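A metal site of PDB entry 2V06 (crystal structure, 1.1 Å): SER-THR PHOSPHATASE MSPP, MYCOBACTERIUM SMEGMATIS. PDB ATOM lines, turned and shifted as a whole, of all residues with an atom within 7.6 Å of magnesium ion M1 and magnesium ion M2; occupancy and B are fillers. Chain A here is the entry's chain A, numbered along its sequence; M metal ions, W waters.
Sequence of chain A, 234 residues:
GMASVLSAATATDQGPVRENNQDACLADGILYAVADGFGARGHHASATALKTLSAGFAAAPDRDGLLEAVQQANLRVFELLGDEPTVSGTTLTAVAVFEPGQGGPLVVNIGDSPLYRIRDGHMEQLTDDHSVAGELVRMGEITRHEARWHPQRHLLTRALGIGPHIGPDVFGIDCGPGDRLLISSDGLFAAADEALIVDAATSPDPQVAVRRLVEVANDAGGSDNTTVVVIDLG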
ATOM      1  N   ARG A  18      26.953 -21.232  21.669  1.00  0.00           N
ATOM      2  CA  ARG A  18      25.680 -20.878  21.068  1.00  0.00           C
ATOM      3  C   ARG A  18      25.504 -19.379  20.932  1.00  0.00           C
ATOM      4  O   ARG A  18      25.916 -18.617  21.790  1.00  0.00           O
ATOM      5  CB  ARG A  18      24.530 -21.454  21.881  1.00  0.00           C
ATOM      6  CG  ARG A  18      24.471 -22.955  22.012  1.00  0.00           C
ATOM      7  CD  ARG A  18      24.529 -23.697  20.656  1.00  0.00           C
ATOM      8  NE  ARG A  18      24.373 -25.138  20.851  1.00  0.00           N
ATOM      9  CZ  ARG A  18      23.288 -25.862  20.749  1.00  0.00           C
ATOM     10  NH1 ARG A  18      22.133 -25.313  20.482  1.00  0.00           N
ATOM     11  NH2 ARG A  18      23.312 -27.194  20.943  1.00  0.00           N
ATOM     12  N   ASN A  20      22.578 -17.834  20.831  1.00  0.00           N
ATOM     13  CA  ASN A  20      21.431 -17.437  21.579  1.00  0.00           C
ATOM     14  C   ASN A  20      21.292 -18.383  22.779  1.00  0.00           C
ATOM     15  O   ASN A  20      21.739 -19.528  22.714  1.00  0.00           O
ATOM     16  CB  ASN A  20      20.088 -17.506  20.800  1.00  0.00           C
ATOM     17  CG  ASN A  20      20.069 -16.413  19.740  1.00  0.00           C
ATOM     18  OD1 ASN A  20      20.457 -16.647  18.598  1.00  0.00           O
ATOM     19  ND2 ASN A  20      19.606 -15.221  20.141  1.00  0.00           N
ATOM     20  N   ASN A  21      20.630 -17.909  23.843  1.00  0.00           N
ATOM     21  CA  ASN A  21      20.207 -18.785  24.913  1.00  0.00           C
ATOM     22  C   ASN A  21      18.714 -19.038  24.647  1.00  0.00           C
ATOM     23  O   ASN A  21      17.861 -18.191  24.904  1.00  0.00           O
ATOM     24  CB  ASN A  21      20.385 -18.167  26.298  1.00  0.00           C
ATOM     25  CG  ASN A  21      20.104 -19.221  27.328  1.00  0.00           C
ATOM     26  OD1 ASN A  21      19.638 -20.312  27.051  1.00  0.00           O
ATOM     27  ND2 ASN A  21      20.383 -18.870  28.593  1.00  0.00           N
ATOM     28  N   GLN A  22      18.437 -20.236  24.142  1.00  0.00           N
ATOM     29  CA  GLN A  22      17.053 -20.612  23.824  1.00  0.00           C
ATOM     30  C   GLN A  22      16.436 -21.452  24.940  1.00  0.00           C
ATOM     31  O   GLN A  22      15.319 -21.946  24.748  1.00  0.00           O
ATOM     32  CB  GLN A  22      16.959 -21.307  22.502  1.00  0.00           C
ATOM     33  CG  GLN A  22      17.606 -20.524  21.355  1.00  0.00           C
ATOM     34  CD  GLN A  22      17.287 -21.151  20.009  1.00  0.00           C
ATOM     35  OE1 GLN A  22      17.412 -22.366  19.865  1.00  0.00           O
ATOM     36  NE2 GLN A  22      16.952 -20.312  19.055  1.00  0.00           N
ATOM     37  N   ASP A  23      17.119 -21.625  26.039  1.00  0.00           N
ATOM     38  CA  ASP A  23      16.548 -22.256  27.203  1.00  0.00           C
ATOM     39  C   ASP A  23      15.768 -21.225  28.006  1.00  0.00           C
ATOM     40  O   ASP A  23      16.015 -20.004  27.968  1.00  0.00           O
ATOM     41  CB  ASP A  23      17.613 -22.824  28.136  1.00  0.00           C
ATOM     42  CG  ASP A  23      18.337 -24.104  27.752  1.00  0.00           C
ATOM     43  OD1 ASP A  23      18.045 -24.715  26.696  1.00  0.00           O
ATOM     44  OD2 ASP A  23      19.206 -24.505  28.576  1.00  0.00           O
ATOM     45  N   ALA A  35      12.436 -25.320  29.886  1.00  0.00           N
ATOM     46  CA  ALA A  35      12.031 -25.429  28.494  1.00  0.00           C
ATOM     47  C   ALA A  35      13.277 -25.179  27.618  1.00  0.00           C
ATOM     48  O   ALA A  35      13.873 -24.090  27.758  1.00  0.00           O
ATOM     49  CB  ALA A  35      10.905 -24.510  28.129  1.00  0.00           C
ATOM     50  N   ASP A  36      13.653 -26.119  26.798  1.00  0.00           N
ATOM     51  CA  ASP A  36      14.776 -25.986  25.880  1.00  0.00           C
ATOM     52  C   ASP A  36      14.230 -25.757  24.482  1.00  0.00           C
ATOM     53  O   ASP A  36      13.758 -26.687  23.824  1.00  0.00           O
ATOM     54  CB  ASP A  36      15.652 -27.261  25.968  1.00  0.00           C
ATOM     55  CG  ASP A  36      16.866 -27.208  25.068  1.00  0.00           C
ATOM     56  OD1 ASP A  36      16.889 -26.324  24.178  1.00  0.00           O
ATOM     57  OD2 ASP A  36      17.770 -28.067  25.217  1.00  0.00           O
ATOM     58  N   GLY A  37      14.322 -24.524  24.022  1.00  0.00           N
ATOM     59  CA  GLY A  37      13.874 -24.160  22.694  1.00  0.00           C
ATOM     60  C   GLY A  37      14.881 -24.571  21.640  1.00  0.00           C
ATOM     61  O   GLY A  37      16.071 -24.679  21.871  1.00  0.00           O
ATOM     62  N   PHE A  38      14.328 -24.746  20.427  1.00  0.00           N
ATOM     63  CA  PHE A  38      15.120 -25.038  19.238  1.00  0.00           C
ATOM     64  C   PHE A  38      14.588 -24.240  18.061  1.00  0.00           C
ATOM     65  O   PHE A  38      13.387 -23.918  18.035  1.00  0.00           O
ATOM     66  CB  PHE A  38      15.160 -26.524  18.936  1.00  0.00           C
ATOM     67  CG  PHE A  38      13.876 -27.120  18.400  1.00  0.00           C
ATOM     68  CD1 PHE A  38      13.523 -27.120  17.064  1.00  0.00           C
ATOM     69  CD2 PHE A  38      13.002 -27.728  19.289  1.00  0.00           C
ATOM     70  CE1 PHE A  38      12.359 -27.651  16.622  1.00  0.00           C
ATOM     71  CE2 PHE A  38      11.821 -28.314  18.869  1.00  0.00           C
ATOM     72  CZ  PHE A  38      11.542 -28.282  17.503  1.00  0.00           C
ATOM     73  N   GLY A  39      15.439 -24.053  17.066  1.00  0.00           N
ATOM     74  CA  GLY A  39      15.038 -23.420  15.809  1.00  0.00           C
ATOM     75  C   GLY A  39      15.267 -21.924  15.781  1.00  0.00           C
ATOM     76  O   GLY A  39      15.743 -21.340  16.764  1.00  0.00           O
ATOM     77  N   GLY A  42      13.528 -20.449  18.656  1.00  0.00           N
ATOM     78  CA  GLY A  42      13.512 -21.306  19.832  1.00  0.00           C
ATOM     79  C   GLY A  42      13.378 -20.565  21.131  1.00  0.00           C
ATOM     80  O   GLY A  42      12.755 -21.021  22.066  1.00  0.00           O
ATOM     81  N   HIS A  43      13.933 -19.387  21.216  1.00  0.00           N
ATOM     82  CA  HIS A  43      13.766 -18.523  22.381  1.00  0.00           C
ATOM     83  C   HIS A  43      12.329 -18.161  22.618  1.00  0.00           C
ATOM     84  O   HIS A  43      11.783 -18.201  23.721  1.00  0.00           O
ATOM     85  CB  HIS A  43      14.689 -17.330  22.221  1.00  0.00           C
ATOM     86  CG  HIS A  43      14.489 -16.379  21.087  1.00  0.00           C
ATOM     87  ND1 HIS A  43      14.109 -16.691  19.771  1.00  0.00           N
ATOM     88  CD2 HIS A  43      14.624 -15.032  21.066  1.00  0.00           C
ATOM     89  CE1 HIS A  43      14.069 -15.590  19.060  1.00  0.00           C
ATOM     90  NE2 HIS A  43      14.353 -14.549  19.815  1.00  0.00           N
ATOM     91  N   SER A  46      10.363 -21.320  23.921  1.00  0.00           N
ATOM     92  CA  SER A  46      10.556 -21.680  25.348  1.00  0.00           C
ATOM     93  C   SER A  46       9.963 -20.612  26.248  1.00  0.00           C
ATOM     94  O   SER A  46       9.268 -20.900  27.239  1.00  0.00           O
ATOM     95  CB  SER A  46      12.022 -21.998  25.628  1.00  0.00           C
ATOM     96  OG  SER A  46      12.779 -20.876  25.316  1.00  0.00           O
ATOM     97  N   GLY A  89      10.410 -24.899  18.122  1.00  0.00           N
ATOM     98  CA  GLY A  89       9.597 -25.468  19.188  1.00  0.00           C
ATOM     99  C   GLY A  89      10.409 -25.542  20.440  1.00  0.00           C
ATOM    100  O   GLY A  89      11.457 -24.946  20.575  1.00  0.00           O
ATOM    101  N   THR A  90       9.911 -26.331  21.427  1.00  0.00           N
ATOM    102  CA  THR A  90      10.630 -26.418  22.679  1.00  0.00           C
ATOM    103  C   THR A  90      10.334 -27.715  23.373  1.00  0.00           C
ATOM    104  O   THR A  90       9.250 -28.279  23.227  1.00  0.00           O
ATOM    105  CB  THR A  90      10.248 -25.220  23.563  1.00  0.00           C
ATOM    106  OG1 THR A  90      11.078 -25.202  24.737  1.00  0.00           O
ATOM    107  CG2 THR A  90       8.796 -25.175  23.970  1.00  0.00           C
ATOM    108  N   THR A  91      11.248 -28.158  24.214  1.00  0.00           N
ATOM    109  CA  THR A  91      10.952 -29.153  25.202  1.00  0.00           C
ATOM    110  C   THR A  91      10.227 -28.478  26.360  1.00  0.00           C
ATOM    111  O   THR A  91      10.254 -27.255  26.485  1.00  0.00           O
ATOM    112  CB  THR A  91      12.231 -29.821  25.724  1.00  0.00           C
ATOM    113  OG1 THR A  91      12.877 -28.867  26.596  1.00  0.00           O
ATOM    114  CG2 THR A  91      13.189 -30.276  24.646  1.00  0.00           C
ATOM    115  N   ASP A 112      13.615 -33.720  25.937  1.00  0.00           N
ATOM    116  CA  ASP A 112      14.822 -34.293  26.511  1.00  0.00           C
ATOM    117  C   ASP A 112      15.489 -33.429  27.569  1.00  0.00           C
ATOM    118  O   ASP A 112      16.695 -33.475  27.751  1.00  0.00           O
ATOM    119  CB  ASP A 112      15.851 -34.594  25.391  1.00  0.00           C
ATOM    120  CG  ASP A 112      16.461 -33.344  24.775  1.00  0.00           C
ATOM    121  OD1 ASP A 112      15.934 -32.216  25.014  1.00  0.00           O
ATOM    122  OD2 ASP A 112      17.499 -33.446  24.133  1.00  0.00           O
ATOM    123  N   SER A 113      14.664 -32.683  28.355  1.00  0.00           N
ATOM    124  CA  SER A 113      15.207 -31.920  29.457  1.00  0.00           C
ATOM    125  C   SER A 113      14.976 -32.715  30.739  1.00  0.00           C
ATOM    126  O   SER A 113      13.823 -32.691  31.246  1.00  0.00           O
ATOM    127  CB  SER A 113      14.505 -30.588  29.517  1.00  0.00           C
ATOM    128  OG  SER A 113      14.695 -29.835  28.313  1.00  0.00           O
ATOM    129  N   ARG A 153      21.027 -38.354  19.580  1.00  0.00           N
ATOM    130  CA  ARG A 153      20.338 -37.855  20.762  1.00  0.00           C
ATOM    131  C   ARG A 153      19.712 -36.471  20.547  1.00  0.00           C
ATOM    132  O   ARG A 153      18.812 -36.028  21.239  1.00  0.00           O
ATOM    133  CB  ARG A 153      21.259 -37.798  21.980  1.00  0.00           C
ATOM    134  CG  ARG A 153      22.108 -36.567  22.090  1.00  0.00           C
ATOM    135  CD  ARG A 153      22.644 -36.480  23.507  1.00  0.00           C
ATOM    136  NE  ARG A 153      23.473 -35.291  23.702  1.00  0.00           N
ATOM    137  CZ  ARG A 153      22.947 -34.087  23.933  1.00  0.00           C
ATOM    138  NH1 ARG A 153      21.633 -33.886  23.995  1.00  0.00           N
ATOM    139  NH2 ARG A 153      23.742 -33.051  24.116  1.00  0.00           N
ATOM    140  N   HIS A 154      20.113 -35.766  19.520  1.00  0.00           N
ATOM    141  CA  HIS A 154      19.572 -34.430  19.318  1.00  0.00           C
ATOM    142  C   HIS A 154      18.325 -34.431  18.473  1.00  0.00           C
ATOM    143  O   HIS A 154      17.739 -33.371  18.249  1.00  0.00           O
ATOM    144  CB  HIS A 154      20.630 -33.575  18.606  1.00  0.00           C
ATOM    145  CG  HIS A 154      21.763 -33.226  19.506  1.00  0.00           C
ATOM    146  ND1 HIS A 154      21.704 -32.315  20.533  1.00  0.00           N
ATOM    147  CD2 HIS A 154      23.028 -33.718  19.513  1.00  0.00           C
ATOM    148  CE1 HIS A 154      22.869 -32.254  21.126  1.00  0.00           C
ATOM    149  NE2 HIS A 154      23.703 -33.103  20.525  1.00  0.00           N
ATOM    150  N   SER A 185      18.172 -28.712  31.339  1.00  0.00           N
ATOM    151  CA  SER A 185      18.256 -28.928  29.913  1.00  0.00           C
ATOM    152  C   SER A 185      19.365 -29.937  29.624  1.00  0.00           C
ATOM    153  O   SER A 185      20.247 -30.198  30.471  1.00  0.00           O
ATOM    154  CB  SER A 185      18.463 -27.629  29.129  1.00  0.00           C
ATOM    155  OG  SER A 185      19.677 -27.037  29.446  1.00  0.00           O
ATOM    156  N   ASP A 186      19.366 -30.471  28.416  1.00  0.00           N
ATOM    157  CA  ASP A 186      20.405 -31.386  27.957  1.00  0.00           C
ATOM    158  C   ASP A 186      21.808 -30.805  27.993  1.00  0.00           C
ATOM    159  O   ASP A 186      22.793 -31.567  27.945  1.00  0.00           O
ATOM    160  CB  ASP A 186      20.014 -31.953  26.602  1.00  0.00           C
ATOM    161  CG  ASP A 186      20.094 -30.962  25.467  1.00  0.00           C
ATOM    162  OD1 ASP A 186      19.906 -29.732  25.684  1.00  0.00           O
ATOM    163  OD2 ASP A 186      20.376 -31.420  24.319  1.00  0.00           O
ATOM    164  N   GLY A 187      21.973 -29.491  28.021  1.00  0.00           N
ATOM    165  CA  GLY A 187      23.308 -28.905  27.973  1.00  0.00           C
ATOM    166  C   GLY A 187      24.151 -29.324  29.138  1.00  0.00           C
ATOM    167  O   GLY A 187      25.390 -29.382  29.006  1.00  0.00           O
ATOM    168  N   LEU A 188      23.544 -29.656  30.289  1.00  0.00           N
ATOM    169  CA  LEU A 188      24.379 -30.001  31.460  1.00  0.00           C
ATOM    170  C   LEU A 188      25.239 -31.237  31.156  1.00  0.00           C
ATOM    171  O   LEU A 188      26.383 -31.301  31.613  1.00  0.00           O
ATOM    172  CB  LEU A 188      23.439 -30.263  32.629  1.00  0.00           C
ATOM    173  CG  LEU A 188      24.104 -30.716  33.924  1.00  0.00           C
ATOM    174  CD1 LEU A 188      25.136 -29.746  34.395  1.00  0.00           C
ATOM    175  CD2 LEU A 188      23.061 -30.930  34.978  1.00  0.00           C
ATOM    176  N   ASP A 224      26.339 -26.308  24.495  1.00  0.00           N
ATOM    177  CA  ASP A 224      24.933 -25.936  24.476  1.00  0.00           C
ATOM    178  C   ASP A 224      24.642 -24.942  25.623  1.00  0.00           C
ATOM    179  O   ASP A 224      25.432 -24.778  26.523  1.00  0.00           O
ATOM    180  CB  ASP A 224      24.028 -27.173  24.565  1.00  0.00           C
ATOM    181  CG  ASP A 224      22.553 -27.004  24.208  1.00  0.00           C
ATOM    182  OD1 ASP A 224      22.153 -25.912  23.713  1.00  0.00           O
ATOM    183  OD2 ASP A 224      21.832 -28.013  24.380  1.00  0.00           O
ATOM    184  N   ASN A 225      23.470 -24.330  25.520  1.00  0.00           N
ATOM    185  CA  ASN A 225      22.880 -23.643  26.684  1.00  0.00           C
ATOM    186  C   ASN A 225      22.687 -24.691  27.800  1.00  0.00           C
ATOM    187  O   ASN A 225      22.274 -25.835  27.520  1.00  0.00           O
ATOM    188  CB  ASN A 225      21.539 -23.071  26.343  1.00  0.00           C
ATOM    189  CG  ASN A 225      21.498 -22.254  25.048  1.00  0.00           C
ATOM    190  OD1 ASN A 225      20.490 -22.288  24.332  1.00  0.00           O
ATOM    191  ND2 ASN A 225      22.550 -21.486  24.782  1.00  0.00           N
ATOM    192  N   THR A 226      22.886 -24.261  29.045  1.00  0.00           N
ATOM    193  CA  THR A 226      22.655 -25.132  30.219  1.00  0.00           C
ATOM    194  C   THR A 226      21.753 -24.368  31.159  1.00  0.00           C
ATOM    195  O   THR A 226      22.040 -23.232  31.522  1.00  0.00           O
ATOM    196  CB  THR A 226      23.965 -25.498  30.925  1.00  0.00           C
ATOM    197  OG1 THR A 226      24.767 -26.280  30.035  1.00  0.00           O
ATOM    198  CG2 THR A 226      23.658 -26.311  32.183  1.00  0.00           C
HETATM  199 MG    MG M   1      19.741 -28.070  24.617  1.00  0.00          MG
HETATM  200 MG    MG M   2      17.864 -25.447  22.654  1.00  0.00          MG
HETATM  201  O   HOH W   1      18.808 -24.301  21.227  1.00  0.00           O
HETATM  202  O   HOH W   2      19.338 -29.372  23.018  1.00  0.00           O
HETATM  203  O   HOH W   3      18.325 -24.015  24.088  1.00  0.00           O
HETATM  204  O   HOH W   4      17.521 -27.081  21.432  1.00  0.00           O
HETATM  205  O   HOH W   5      20.005 -26.640  26.131  1.00  0.00           O
HETATM  206  O   HOH W   6      19.698 -26.485  23.084  1.00  0.00           O
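The nearest printed residue that does not touch magnesium ion M1 is Asp 23 (4.3 Å).
Magnesium ion M2 is bound by the side-chain carboxylate (OD1) of Asp 36 (2.0 Å), water W1 (2.1 Å), water W4 (2.1 Å), water W3 (2.1 Å), the backbone carbonyl oxygen (O) of Gly 37 (2.1 Å) and water W6 (2.2 Å).
Magnesium ion M2 has six donor atoms within binding distance.
OD2 of Asp 186 is in salt-bridge range of NH1 of Arg 153 (2.8 Å).
The backbone NH (N) of Asp 36 sits at hydrogen-bond distance from the side-chain hydroxyl (OG1) of Thr 91 (2.9 Å).
OG1 of Thr 90 sits at hydrogen-bond distance from O of Asp 36, 3.2 Å away.
O of Gln 22 lies within hydrogen-bond range of N of Gly 37 (2.9 Å).
The side-chain hydroxyl (OG1) of Thr 90 is in hydrogen-bond range of the backbone NH (N) of Gly 37 (3.4 Å).
The side-chain carboxylate (OD1) of Asp 224 is in salt-bridge range of the guanidinium group (NH2) of Arg 18.
Water W3 bridges the side-chain carboxylate of Asp 23 (2.7 Å) and the side-chain amide oxygen of Asn 225 (2.8 Å).
Magnesium ion M1 is bound by OD1 of Asp 186 (2.0 Å), OD2 of Asp 36 (2.1 Å), water W5 (2.1 Å), water W2 (2.1 Å), OD2 of Asp 224 (2.1 Å) and water W6 (2.2 Å).
Along chain A the residues within 4 Å of magnesium ion M2 span positions 36 to 37.
The nearest printed residue that does not touch magnesium ion M2 is Asp 23 (4.1 Å).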
